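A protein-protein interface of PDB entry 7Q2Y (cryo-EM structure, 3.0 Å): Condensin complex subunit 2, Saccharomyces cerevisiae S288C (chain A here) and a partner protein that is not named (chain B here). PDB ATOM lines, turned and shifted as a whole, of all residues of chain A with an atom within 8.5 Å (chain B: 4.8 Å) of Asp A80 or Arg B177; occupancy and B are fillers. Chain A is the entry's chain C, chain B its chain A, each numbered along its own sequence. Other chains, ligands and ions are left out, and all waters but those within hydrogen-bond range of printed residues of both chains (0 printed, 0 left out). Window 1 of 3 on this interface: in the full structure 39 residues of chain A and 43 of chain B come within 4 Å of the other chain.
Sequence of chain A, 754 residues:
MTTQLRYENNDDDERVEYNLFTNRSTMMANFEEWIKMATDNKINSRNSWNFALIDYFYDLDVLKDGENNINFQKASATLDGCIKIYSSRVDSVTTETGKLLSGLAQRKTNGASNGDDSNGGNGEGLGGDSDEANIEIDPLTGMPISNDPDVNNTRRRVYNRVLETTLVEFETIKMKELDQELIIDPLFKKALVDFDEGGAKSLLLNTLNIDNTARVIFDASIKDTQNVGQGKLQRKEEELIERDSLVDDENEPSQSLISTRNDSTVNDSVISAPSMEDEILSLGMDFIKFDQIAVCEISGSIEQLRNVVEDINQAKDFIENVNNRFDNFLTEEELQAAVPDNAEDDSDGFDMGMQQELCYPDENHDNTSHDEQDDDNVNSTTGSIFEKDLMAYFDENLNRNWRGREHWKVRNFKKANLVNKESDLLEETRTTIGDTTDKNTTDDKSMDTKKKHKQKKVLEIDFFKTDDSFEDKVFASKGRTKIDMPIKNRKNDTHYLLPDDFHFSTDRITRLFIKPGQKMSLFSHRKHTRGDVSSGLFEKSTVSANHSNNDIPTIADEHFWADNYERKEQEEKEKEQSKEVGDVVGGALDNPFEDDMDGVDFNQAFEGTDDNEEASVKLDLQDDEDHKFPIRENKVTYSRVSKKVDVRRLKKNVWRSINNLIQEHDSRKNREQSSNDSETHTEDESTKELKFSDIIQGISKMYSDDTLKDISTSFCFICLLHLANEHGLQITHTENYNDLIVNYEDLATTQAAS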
ATOM      1  N   TRP A  34     -25.122  27.669 -17.445  1.00  0.00           N
ATOM      2  CA  TRP A  34     -24.306  28.298 -18.479  1.00  0.00           C
ATOM      3  C   TRP A  34     -24.445  27.577 -19.815  1.00  0.00           C
ATOM      4  O   TRP A  34     -24.498  28.223 -20.868  1.00  0.00           O
ATOM      5  CB  TRP A  34     -22.845  28.353 -18.036  1.00  0.00           C
ATOM      6  CG  TRP A  34     -22.613  29.284 -16.884  1.00  0.00           C
ATOM      7  CD1 TRP A  34     -23.436  30.289 -16.467  1.00  0.00           C
ATOM      8  CD2 TRP A  34     -21.484  29.299 -16.003  1.00  0.00           C
ATOM      9  NE1 TRP A  34     -22.890  30.927 -15.380  1.00  0.00           N
ATOM     10  CE2 TRP A  34     -21.691  30.339 -15.076  1.00  0.00           C
ATOM     11  CE3 TRP A  34     -20.318  28.534 -15.907  1.00  0.00           C
ATOM     12  CZ2 TRP A  34     -20.777  30.633 -14.067  1.00  0.00           C
ATOM     13  CZ3 TRP A  34     -19.412  28.828 -14.906  1.00  0.00           C
ATOM     14  CH2 TRP A  34     -19.646  29.867 -13.999  1.00  0.00           C
ATOM     15  N   ILE A  35     -24.510  26.243 -19.800  1.00  0.00           N
ATOM     16  CA  ILE A  35     -24.731  25.508 -21.043  1.00  0.00           C
ATOM     17  C   ILE A  35     -26.110  25.821 -21.614  1.00  0.00           C
ATOM     18  O   ILE A  35     -26.272  25.974 -22.831  1.00  0.00           O
ATOM     19  CB  ILE A  35     -24.534  23.996 -20.823  1.00  0.00           C
ATOM     20  CG1 ILE A  35     -23.100  23.702 -20.379  1.00  0.00           C
ATOM     21  CG2 ILE A  35     -24.865  23.219 -22.089  1.00  0.00           C
ATOM     22  CD1 ILE A  35     -22.051  24.118 -21.386  1.00  0.00           C
ATOM     23  N   ALA A  38     -25.868  29.225 -23.211  1.00  0.00           N
ATOM     24  CA  ALA A  38     -25.130  29.151 -24.468  1.00  0.00           C
ATOM     25  C   ALA A  38     -25.985  28.550 -25.575  1.00  0.00           C
ATOM     26  O   ALA A  38     -25.946  29.013 -26.721  1.00  0.00           O
ATOM     27  CB  ALA A  38     -23.848  28.340 -24.277  1.00  0.00           C
ATOM     28  N   THR A  39     -26.757  27.509 -25.255  1.00  0.00           N
ATOM     29  CA  THR A  39     -27.663  26.927 -26.242  1.00  0.00           C
ATOM     30  C   THR A  39     -28.742  27.923 -26.649  1.00  0.00           C
ATOM     31  O   THR A  39     -29.111  28.007 -27.827  1.00  0.00           O
ATOM     32  CB  THR A  39     -28.291  25.648 -25.686  1.00  0.00           C
ATOM     33  OG1 THR A  39     -27.258  24.702 -25.381  1.00  0.00           O
ATOM     34  CG2 THR A  39     -29.246  25.033 -26.700  1.00  0.00           C
ATOM     35  N   ASN A  41     -28.461  30.994 -26.952  1.00  0.00           N
ATOM     36  CA  ASN A  41     -27.851  32.115 -27.673  1.00  0.00           C
ATOM     37  C   ASN A  41     -28.105  33.439 -26.953  1.00  0.00           C
ATOM     38  O   ASN A  41     -28.340  34.478 -27.574  1.00  0.00           O
ATOM     39  CB  ASN A  41     -28.346  32.174 -29.122  1.00  0.00           C
ATOM     40  CG  ASN A  41     -27.377  31.537 -30.095  1.00  0.00           C
ATOM     41  OD1 ASN A  41     -26.295  31.096 -29.711  1.00  0.00           O
ATOM     42  ND2 ASN A  41     -27.760  31.487 -31.366  1.00  0.00           N
ATOM     43  N   ILE A  43     -25.809  34.670 -24.723  1.00  0.00           N
ATOM     44  CA  ILE A  43     -24.521  35.234 -24.334  1.00  0.00           C
ATOM     45  C   ILE A  43     -24.154  36.353 -25.299  1.00  0.00           C
ATOM     46  O   ILE A  43     -24.176  36.167 -26.522  1.00  0.00           O
ATOM     47  CB  ILE A  43     -23.436  34.146 -24.304  1.00  0.00           C
ATOM     48  CG1 ILE A  43     -23.770  33.090 -23.247  1.00  0.00           C
ATOM     49  CG2 ILE A  43     -22.071  34.757 -24.033  1.00  0.00           C
ATOM     50  CD1 ILE A  43     -22.898  31.858 -23.321  1.00  0.00           C
ATOM     51  N   LEU A  53     -16.968  29.858 -17.918  1.00  0.00           N
ATOM     52  CA  LEU A  53     -16.947  28.403 -17.972  1.00  0.00           C
ATOM     53  C   LEU A  53     -15.697  27.861 -18.650  1.00  0.00           C
ATOM     54  O   LEU A  53     -15.542  26.639 -18.751  1.00  0.00           O
ATOM     55  CB  LEU A  53     -18.207  27.878 -18.676  1.00  0.00           C
ATOM     56  CG  LEU A  53     -18.507  28.254 -20.132  1.00  0.00           C
ATOM     57  CD1 LEU A  53     -17.821  27.321 -21.124  1.00  0.00           C
ATOM     58  CD2 LEU A  53     -20.009  28.281 -20.376  1.00  0.00           C
ATOM     59  N   PHE A  57     -13.917  24.269 -18.386  1.00  0.00           N
ATOM     60  CA  PHE A  57     -13.441  23.521 -19.546  1.00  0.00           C
ATOM     61  C   PHE A  57     -12.013  23.037 -19.336  1.00  0.00           C
ATOM     62  O   PHE A  57     -11.662  21.919 -19.731  1.00  0.00           O
ATOM     63  CB  PHE A  57     -13.541  24.385 -20.802  1.00  0.00           C
ATOM     64  CG  PHE A  57     -13.322  23.629 -22.082  1.00  0.00           C
ATOM     65  CD1 PHE A  57     -13.816  22.345 -22.240  1.00  0.00           C
ATOM     66  CD2 PHE A  57     -12.633  24.207 -23.136  1.00  0.00           C
ATOM     67  CE1 PHE A  57     -13.620  21.650 -23.419  1.00  0.00           C
ATOM     68  CE2 PHE A  57     -12.434  23.519 -24.317  1.00  0.00           C
ATOM     69  CZ  PHE A  57     -12.931  22.240 -24.460  1.00  0.00           C
ATOM     70  N   PHE A  72     -18.455  13.208 -24.664  1.00  0.00           N
ATOM     71  CA  PHE A  72     -18.116  14.096 -25.770  1.00  0.00           C
ATOM     72  C   PHE A  72     -19.252  15.051 -26.110  1.00  0.00           C
ATOM     73  O   PHE A  72     -19.010  16.101 -26.715  1.00  0.00           O
ATOM     74  CB  PHE A  72     -17.710  13.278 -26.992  1.00  0.00           C
ATOM     75  CG  PHE A  72     -16.253  12.932 -27.015  1.00  0.00           C
ATOM     76  CD1 PHE A  72     -15.686  12.221 -25.972  1.00  0.00           C
ATOM     77  CD2 PHE A  72     -15.447  13.324 -28.069  1.00  0.00           C
ATOM     78  CE1 PHE A  72     -14.345  11.903 -25.980  1.00  0.00           C
ATOM     79  CE2 PHE A  72     -14.106  13.009 -28.081  1.00  0.00           C
ATOM     80  CZ  PHE A  72     -13.555  12.298 -27.034  1.00  0.00           C
ATOM     81  N   GLN A  73     -20.485  14.716 -25.745  1.00  0.00           N
ATOM     82  CA  GLN A  73     -21.595  15.671 -25.927  1.00  0.00           C
ATOM     83  C   GLN A  73     -21.390  16.840 -24.964  1.00  0.00           C
ATOM     84  O   GLN A  73     -21.602  17.977 -25.412  1.00  0.00           O
ATOM     85  CB  GLN A  73     -22.939  14.950 -25.826  1.00  0.00           C
ATOM     86  CG  GLN A  73     -23.341  14.244 -27.110  1.00  0.00           C
ATOM     87  CD  GLN A  73     -22.671  12.900 -27.248  1.00  0.00           C
ATOM     88  OE1 GLN A  73     -21.477  12.805 -27.519  1.00  0.00           O
ATOM     89  NE2 GLN A  73     -23.443  11.842 -27.059  1.00  0.00           N
ATOM     90  N   LYS A  74     -20.983  16.608 -23.706  1.00  0.00           N
ATOM     91  CA  LYS A  74     -20.649  17.684 -22.783  1.00  0.00           C
ATOM     92  C   LYS A  74     -19.411  18.438 -23.249  1.00  0.00           C
ATOM     93  O   LYS A  74     -19.325  19.659 -23.093  1.00  0.00           O
ATOM     94  CB  LYS A  74     -20.443  17.123 -21.376  1.00  0.00           C
ATOM     95  CG  LYS A  74     -21.703  16.545 -20.751  1.00  0.00           C
ATOM     96  CD  LYS A  74     -21.449  16.062 -19.333  1.00  0.00           C
ATOM     97  CE  LYS A  74     -22.685  15.400 -18.746  1.00  0.00           C
ATOM     98  NZ  LYS A  74     -23.794  16.373 -18.542  1.00  0.00           N
ATOM     99  N   ALA A  75     -18.439  17.724 -23.824  1.00  0.00           N
ATOM    100  CA  ALA A  75     -17.248  18.383 -24.350  1.00  0.00           C
ATOM    101  C   ALA A  75     -17.598  19.334 -25.488  1.00  0.00           C
ATOM    102  O   ALA A  75     -17.071  20.451 -25.558  1.00  0.00           O
ATOM    103  CB  ALA A  75     -16.232  17.341 -24.815  1.00  0.00           C
ATOM    104  N   SER A  76     -18.485  18.909 -26.390  1.00  0.00           N
ATOM    105  CA  SER A  76     -18.913  19.781 -27.478  1.00  0.00           C
ATOM    106  C   SER A  76     -19.674  20.988 -26.948  1.00  0.00           C
ATOM    107  O   SER A  76     -19.498  22.108 -27.443  1.00  0.00           O
ATOM    108  CB  SER A  76     -19.771  18.997 -28.471  1.00  0.00           C
ATOM    109  OG  SER A  76     -18.985  18.081 -29.212  1.00  0.00           O
ATOM    110  N   ALA A  77     -20.527  20.781 -25.941  1.00  0.00           N
ATOM    111  CA  ALA A  77     -21.237  21.907 -25.342  1.00  0.00           C
ATOM    112  C   ALA A  77     -20.267  22.900 -24.712  1.00  0.00           C
ATOM    113  O   ALA A  77     -20.420  24.119 -24.868  1.00  0.00           O
ATOM    114  CB  ALA A  77     -22.241  21.402 -24.305  1.00  0.00           C
ATOM    115  N   THR A  78     -19.255  22.395 -24.000  1.00  0.00           N
ATOM    116  CA  THR A  78     -18.253  23.268 -23.398  1.00  0.00           C
ATOM    117  C   THR A  78     -17.468  24.024 -24.460  1.00  0.00           C
ATOM    118  O   THR A  78     -17.168  25.210 -24.290  1.00  0.00           O
ATOM    119  CB  THR A  78     -17.299  22.461 -22.520  1.00  0.00           C
ATOM    120  OG1 THR A  78     -16.710  21.408 -23.293  1.00  0.00           O
ATOM    121  CG2 THR A  78     -18.027  21.872 -21.336  1.00  0.00           C
ATOM    122  N   LEU A  79     -17.104  23.348 -25.551  1.00  0.00           N
ATOM    123  CA  LEU A  79     -16.380  24.020 -26.625  1.00  0.00           C
ATOM    124  C   LEU A  79     -17.228  25.118 -27.252  1.00  0.00           C
ATOM    125  O   LEU A  79     -16.725  26.214 -27.535  1.00  0.00           O
ATOM    126  CB  LEU A  79     -15.942  22.999 -27.676  1.00  0.00           C
ATOM    127  CG  LEU A  79     -14.855  23.414 -28.672  1.00  0.00           C
ATOM    128  CD1 LEU A  79     -14.009  22.212 -29.059  1.00  0.00           C
ATOM    129  CD2 LEU A  79     -15.472  24.043 -29.910  1.00  0.00           C
ATOM    130  N   ASP A  80     -18.516  24.846 -27.468  1.00  0.00           N
ATOM    131  CA  ASP A  80     -19.409  25.859 -28.022  1.00  0.00           C
ATOM    132  C   ASP A  80     -19.504  27.064 -27.096  1.00  0.00           C
ATOM    133  O   ASP A  80     -19.405  28.216 -27.539  1.00  0.00           O
ATOM    134  CB  ASP A  80     -20.794  25.257 -28.261  1.00  0.00           C
ATOM    135  CG  ASP A  80     -20.791  24.205 -29.348  1.00  0.00           C
ATOM    136  OD1 ASP A  80     -19.944  24.294 -30.260  1.00  0.00           O
ATOM    137  OD2 ASP A  80     -21.634  23.284 -29.289  1.00  0.00           O
ATOM    138  N   GLY A  81     -19.685  26.812 -25.797  1.00  0.00           N
ATOM    139  CA  GLY A  81     -19.757  27.908 -24.846  1.00  0.00           C
ATOM    140  C   GLY A  81     -18.473  28.710 -24.781  1.00  0.00           C
ATOM    141  O   GLY A  81     -18.502  29.942 -24.724  1.00  0.00           O
ATOM    142  N   CYS A  82     -17.326  28.024 -24.794  1.00  0.00           N
ATOM    143  CA  CYS A  82     -16.043  28.715 -24.744  1.00  0.00           C
ATOM    144  C   CYS A  82     -15.831  29.581 -25.977  1.00  0.00           C
ATOM    145  O   CYS A  82     -15.375  30.723 -25.866  1.00  0.00           O
ATOM    146  CB  CYS A  82     -14.904  27.706 -24.602  1.00  0.00           C
ATOM    147  SG  CYS A  82     -14.770  26.955 -22.967  1.00  0.00           S
ATOM    148  N   ILE A  83     -16.158  29.059 -27.161  1.00  0.00           N
ATOM    149  CA  ILE A  83     -15.989  29.843 -28.380  1.00  0.00           C
ATOM    150  C   ILE A  83     -16.920  31.050 -28.376  1.00  0.00           C
ATOM    151  O   ILE A  83     -16.523  32.158 -28.759  1.00  0.00           O
ATOM    152  CB  ILE A  83     -16.203  28.958 -29.621  1.00  0.00           C
ATOM    153  CG1 ILE A  83     -15.099  27.904 -29.709  1.00  0.00           C
ATOM    154  CG2 ILE A  83     -16.230  29.802 -30.885  1.00  0.00           C
ATOM    155  CD1 ILE A  83     -13.706  28.490 -29.797  1.00  0.00           C
ATOM    156  N   LYS A  84     -18.170  30.858 -27.944  1.00  0.00           N
ATOM    157  CA  LYS A  84     -19.110  31.974 -27.897  1.00  0.00           C
ATOM    158  C   LYS A  84     -18.644  33.049 -26.921  1.00  0.00           C
ATOM    159  O   LYS A  84     -18.702  34.247 -27.229  1.00  0.00           O
ATOM    160  CB  LYS A  84     -20.496  31.461 -27.517  1.00  0.00           C
ATOM    161  CG  LYS A  84     -21.236  30.812 -28.669  1.00  0.00           C
ATOM    162  CD  LYS A  84     -22.722  30.723 -28.400  1.00  0.00           C
ATOM    163  CE  LYS A  84     -23.401  29.854 -29.443  1.00  0.00           C
ATOM    164  NZ  LYS A  84     -23.087  28.412 -29.247  1.00  0.00           N
ATOM    165  N   ILE A  85     -18.166  32.639 -25.745  1.00  0.00           N
ATOM    166  CA  ILE A  85     -17.684  33.599 -24.757  1.00  0.00           C
ATOM    167  C   ILE A  85     -16.436  34.311 -25.265  1.00  0.00           C
ATOM    168  O   ILE A  85     -16.259  35.514 -25.043  1.00  0.00           O
ATOM    169  CB  ILE A  85     -17.438  32.894 -23.411  1.00  0.00           C
ATOM    170  CG1 ILE A  85     -18.769  32.491 -22.777  1.00  0.00           C
ATOM    171  CG2 ILE A  85     -16.652  33.787 -22.462  1.00  0.00           C
ATOM    172  CD1 ILE A  85     -18.625  31.567 -21.596  1.00  0.00           C
ATOM    173  N   TYR A  86     -15.554  33.585 -25.956  1.00  0.00           N
ATOM    174  CA  TYR A  86     -14.357  34.200 -26.517  1.00  0.00           C
ATOM    175  C   TYR A  86     -14.719  35.254 -27.556  1.00  0.00           C
ATOM    176  O   TYR A  86     -14.150  36.353 -27.568  1.00  0.00           O
ATOM    177  CB  TYR A  86     -13.463  33.119 -27.128  1.00  0.00           C
ATOM    178  CG  TYR A  86     -12.097  33.607 -27.548  1.00  0.00           C
ATOM    179  CD1 TYR A  86     -11.070  33.732 -26.624  1.00  0.00           C
ATOM    180  CD2 TYR A  86     -11.832  33.932 -28.872  1.00  0.00           C
ATOM    181  CE1 TYR A  86      -9.820  34.173 -27.003  1.00  0.00           C
ATOM    182  CE2 TYR A  86     -10.583  34.375 -29.260  1.00  0.00           C
ATOM    183  CZ  TYR A  86      -9.581  34.493 -28.322  1.00  0.00           C
ATOM    184  OH  TYR A  86      -8.334  34.934 -28.702  1.00  0.00           O
ATOM    185  N   SER A  87     -15.673  34.936 -28.435  1.00  0.00           N
ATOM    186  CA  SER A  87     -16.111  35.909 -29.433  1.00  0.00           C
ATOM    187  C   SER A  87     -16.750  37.124 -28.773  1.00  0.00           C
ATOM    188  O   SER A  87     -16.504  38.267 -29.182  1.00  0.00           O
ATOM    189  CB  SER A  87     -17.086  35.254 -30.412  1.00  0.00           C
ATOM    190  OG  SER A  87     -16.449  34.234 -31.163  1.00  0.00           O
ATOM    191  N   SER A  88     -17.573  36.898 -27.745  1.00  0.00           N
ATOM    192  CA  SER A  88     -18.203  38.011 -27.043  1.00  0.00           C
ATOM    193  C   SER A  88     -17.164  38.899 -26.368  1.00  0.00           C
ATOM    194  O   SER A  88     -17.280  40.130 -26.389  1.00  0.00           O
ATOM    195  CB  SER A  88     -19.207  37.480 -26.021  1.00  0.00           C
ATOM    196  OG  SER A  88     -20.086  36.537 -26.610  1.00  0.00           O
ATOM    197  N   GLN B 125     -28.301  26.265 -37.660  1.00  0.00           N
ATOM    198  CA  GLN B 125     -27.266  25.711 -36.797  1.00  0.00           C
ATOM    199  C   GLN B 125     -27.881  25.109 -35.542  1.00  0.00           C
ATOM    200  O   GLN B 125     -27.661  23.929 -35.241  1.00  0.00           O
ATOM    201  CB  GLN B 125     -26.248  26.792 -36.436  1.00  0.00           C
ATOM    202  CG  GLN B 125     -25.454  27.311 -37.620  1.00  0.00           C
ATOM    203  CD  GLN B 125     -24.614  26.232 -38.270  1.00  0.00           C
ATOM    204  OE1 GLN B 125     -24.906  25.789 -39.382  1.00  0.00           O
ATOM    205  NE2 GLN B 125     -23.565  25.802 -37.581  1.00  0.00           N
ATOM    206  N   GLN B 129     -26.902  21.320 -34.235  1.00  0.00           N
ATOM    207  CA  GLN B 129     -26.346  20.804 -32.981  1.00  0.00           C
ATOM    208  C   GLN B 129     -27.388  20.065 -32.149  1.00  0.00           C
ATOM    209  O   GLN B 129     -27.038  19.107 -31.451  1.00  0.00           O
ATOM    210  CB  GLN B 129     -25.672  21.881 -32.117  1.00  0.00           C
ATOM    211  CG  GLN B 129     -24.388  22.504 -32.672  1.00  0.00           C
ATOM    212  CD  GLN B 129     -24.623  23.611 -33.660  1.00  0.00           C
ATOM    213  OE1 GLN B 129     -25.709  24.165 -33.728  1.00  0.00           O
ATOM    214  NE2 GLN B 129     -23.598  23.941 -34.439  1.00  0.00           N
ATOM    215  N   MET B 173     -18.913  14.731 -34.436  1.00  0.00           N
ATOM    216  CA  MET B 173     -19.445  15.958 -33.846  1.00  0.00           C
ATOM    217  C   MET B 173     -18.322  16.691 -33.111  1.00  0.00           C
ATOM    218  O   MET B 173     -18.554  17.690 -32.425  1.00  0.00           O
ATOM    219  CB  MET B 173     -20.632  15.645 -32.921  1.00  0.00           C
ATOM    220  CG  MET B 173     -21.333  16.851 -32.308  1.00  0.00           C
ATOM    221  SD  MET B 173     -22.763  16.412 -31.308  1.00  0.00           S
ATOM    222  CE  MET B 173     -23.240  18.023 -30.689  1.00  0.00           C
ATOM    223  N   PHE B 174     -17.092  16.201 -33.257  1.00  0.00           N
ATOM    224  CA  PHE B 174     -15.938  16.784 -32.590  1.00  0.00           C
ATOM    225  C   PHE B 174     -14.863  17.256 -33.556  1.00  0.00           C
ATOM    226  O   PHE B 174     -14.289  18.324 -33.343  1.00  0.00           O
ATOM    227  CB  PHE B 174     -15.336  15.768 -31.610  1.00  0.00           C
ATOM    228  CG  PHE B 174     -14.650  16.392 -30.433  1.00  0.00           C
ATOM    229  CD1 PHE B 174     -13.335  16.812 -30.511  1.00  0.00           C
ATOM    230  CD2 PHE B 174     -15.332  16.565 -29.241  1.00  0.00           C
ATOM    231  CE1 PHE B 174     -12.714  17.384 -29.419  1.00  0.00           C
ATOM    232  CE2 PHE B 174     -14.717  17.138 -28.150  1.00  0.00           C
ATOM    233  CZ  PHE B 174     -13.406  17.549 -28.241  1.00  0.00           C
ATOM    234  N   GLU B 175     -14.604  16.497 -34.625  1.00  0.00           N
ATOM    235  CA  GLU B 175     -13.648  16.926 -35.641  1.00  0.00           C
ATOM    236  C   GLU B 175     -14.108  18.215 -36.310  1.00  0.00           C
ATOM    237  O   GLU B 175     -13.364  19.205 -36.372  1.00  0.00           O
ATOM    238  CB  GLU B 175     -13.479  15.817 -36.684  1.00  0.00           C
ATOM    239  CG  GLU B 175     -12.544  14.685 -36.286  1.00  0.00           C
ATOM    240  CD  GLU B 175     -11.103  14.963 -36.647  1.00  0.00           C
ATOM    241  OE1 GLU B 175     -10.863  15.605 -37.691  1.00  0.00           O
ATOM    242  OE2 GLU B 175     -10.206  14.550 -35.881  1.00  0.00           O
ATOM    243  N   ASP B 176     -15.350  18.223 -36.801  1.00  0.00           N
ATOM    244  CA  ASP B 176     -15.872  19.395 -37.492  1.00  0.00           C
ATOM    245  C   ASP B 176     -15.982  20.586 -36.550  1.00  0.00           C
ATOM    246  O   ASP B 176     -15.720  21.727 -36.949  1.00  0.00           O
ATOM    247  CB  ASP B 176     -17.232  19.078 -38.116  1.00  0.00           C
ATOM    248  CG  ASP B 176     -18.200  18.468 -37.124  1.00  0.00           C
ATOM    249  OD1 ASP B 176     -17.849  17.448 -36.495  1.00  0.00           O
ATOM    250  OD2 ASP B 176     -19.317  19.008 -36.976  1.00  0.00           O
ATOM    251  N   ARG B 177     -16.375  20.345 -35.297  1.00  0.00           N
ATOM    252  CA  ARG B 177     -16.526  21.456 -34.365  1.00  0.00           C
ATOM    253  C   ARG B 177     -15.175  22.031 -33.954  1.00  0.00           C
ATOM    254  O   ARG B 177     -15.048  23.247 -33.782  1.00  0.00           O
ATOM    255  CB  ARG B 177     -17.339  21.032 -33.144  1.00  0.00           C
ATOM    256  CG  ARG B 177     -18.754  20.596 -33.488  1.00  0.00           C
ATOM    257  CD  ARG B 177     -19.591  21.751 -34.029  1.00  0.00           C
ATOM    258  NE  ARG B 177     -19.804  22.813 -33.053  1.00  0.00           N
ATOM    259  CZ  ARG B 177     -20.212  24.036 -33.364  1.00  0.00           C
ATOM    260  NH1 ARG B 177     -20.478  24.382 -34.613  1.00  0.00           N
ATOM    261  NH2 ARG B 177     -20.363  24.936 -32.395  1.00  0.00           N
ATOM    262  N   ARG B 178     -14.148  21.186 -33.801  1.00  0.00           N
ATOM    263  CA  ARG B 178     -12.811  21.730 -33.574  1.00  0.00           C
ATOM    264  C   ARG B 178     -12.339  22.535 -34.775  1.00  0.00           C
ATOM    265  O   ARG B 178     -11.706  23.584 -34.620  1.00  0.00           O
ATOM    266  CB  ARG B 178     -11.787  20.637 -33.259  1.00  0.00           C
ATOM    267  CG  ARG B 178     -11.956  19.924 -31.937  1.00  0.00           C
ATOM    268  CD  ARG B 178     -10.813  18.940 -31.738  1.00  0.00           C
ATOM    269  NE  ARG B 178     -10.859  17.810 -32.657  1.00  0.00           N
ATOM    270  CZ  ARG B 178      -9.965  17.600 -33.611  1.00  0.00           C
ATOM    271  NH1 ARG B 178      -8.967  18.442 -33.822  1.00  0.00           N
ATOM    272  NH2 ARG B 178     -10.074  16.520 -34.375  1.00  0.00           N
ATOM    273  N   GLU B 179     -12.618  22.048 -35.987  1.00  0.00           N
ATOM    274  CA  GLU B 179     -12.206  22.796 -37.172  1.00  0.00           C
ATOM    275  C   GLU B 179     -12.900  24.155 -37.231  1.00  0.00           C
ATOM    276  O   GLU B 179     -12.263  25.178 -37.517  1.00  0.00           O
ATOM    277  CB  GLU B 179     -12.499  21.977 -38.429  1.00  0.00           C
ATOM    278  CG  GLU B 179     -11.642  22.342 -39.627  1.00  0.00           C
ATOM    279  CD  GLU B 179     -12.188  23.521 -40.404  1.00  0.00           C
ATOM    280  OE1 GLU B 179     -13.417  23.738 -40.370  1.00  0.00           O
ATOM    281  OE2 GLU B 179     -11.389  24.228 -41.051  1.00  0.00           O
ATOM    282  N   LYS B 180     -14.204  24.184 -36.940  1.00  0.00           N
ATOM    283  CA  LYS B 180     -14.939  25.446 -36.932  1.00  0.00           C
ATOM    284  C   LYS B 180     -14.436  26.371 -35.831  1.00  0.00           C
ATOM    285  O   LYS B 180     -14.338  27.587 -36.033  1.00  0.00           O
ATOM    286  CB  LYS B 180     -16.436  25.183 -36.771  1.00  0.00           C
ATOM    287  CG  LYS B 180     -17.081  24.508 -37.971  1.00  0.00           C
ATOM    288  CD  LYS B 180     -18.545  24.193 -37.708  1.00  0.00           C
ATOM    289  CE  LYS B 180     -19.388  25.458 -37.688  1.00  0.00           C
ATOM    290  NZ  LYS B 180     -19.461  26.093 -39.034  1.00  0.00           N
ATOM    291  N   ALA B 181     -14.120  25.817 -34.658  1.00  0.00           N
ATOM    292  CA  ALA B 181     -13.576  26.626 -33.574  1.00  0.00           C
ATOM    293  C   ALA B 181     -12.229  27.221 -33.952  1.00  0.00           C
ATOM    294  O   ALA B 181     -11.947  28.382 -33.640  1.00  0.00           O
ATOM    295  CB  ALA B 181     -13.450  25.786 -32.304  1.00  0.00           C
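The side-chain hydroxyl (OG) of Ser A76 is in hydrogen-bond range of the backbone carbonyl oxygen (O) of Met B173, at 3.3 Å.
NE of Arg B177 is in salt-bridge range of OD1 of Asp A80 (3.2 Å).
The side-chain amide nitrogen (NE2) of Gln B129 sits close to the guanidinium group (NH1) of Arg B177 (3.2 Å).
The backbone carbonyl oxygen (O) of Phe A72 lies within hydrogen-bond range of the side-chain hydroxyl (OG) of Ser A76.
The side-chain hydroxyl (OG1) of Thr A78 sits at hydrogen-bond distance from the backbone carbonyl oxygen (O) of Ala A75 (2.5 Å).
The side-chain hydroxyl (OG) of Ser A87 is in hydrogen-bond range of the backbone carbonyl oxygen (O) of Ile A83 (3.2 Å).
Among the printed residues, pairs that only touch across the chains: Phe A72 with Phe B174 (3.4 Å), Leu A79 with Ala B181 (3.6 Å), Ala A75 with Phe B174 (3.7 Å), Ile A83 with Ala B181 (3.7 Å), Ser A76 with Phe B174 (3.96 Å) and Leu A79 with Arg B177 (3.98 Å).
Of chain B, only Arg B177 comes within 4 Å of Asp A80.
Arg B177 touches two residues of chain A.
No residue of chain A comes within 4 Å of Asp B176.
Printed residues of chain B within 4 Å of Ile A83: Ala B181.
Of the printed residues of chain A, Ala B181 touches Leu A79 and Ile A83.
Of the printed residues of chain A, Phe B174 touches Phe A72 (3.4 Å), Ala A75 (3.7 Å) and Ser A76 (3.96 Å).
Of the printed residues of chain B, Phe A72 touches Phe B174.
The nearest residue of chain B that does not touch Asp A80 is Gln B129 (4.4 Å).
The nearest residue of chain A that does not touch Arg B177 is Ser A76 (5.0 Å).
The nearest printed residue of chain A that does not touch Met B173 is Gln A73 (4.8 Å).
Of the 11 printed residues of chain B, 4 touch a printed residue of chain A.
Hydrophobic or aromatic side chains of chain B within 4 Å of the printed part of chain A: Phe B174 and Ala B181.
Among the printed residues, 8 pairs touch across the chains.
Among the printed residues, Asp or Glu carboxylates within 4 Å of a Lys or Arg side-chain nitrogen of the other chain: Asp A80 with Arg B177 (2.3 Å).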
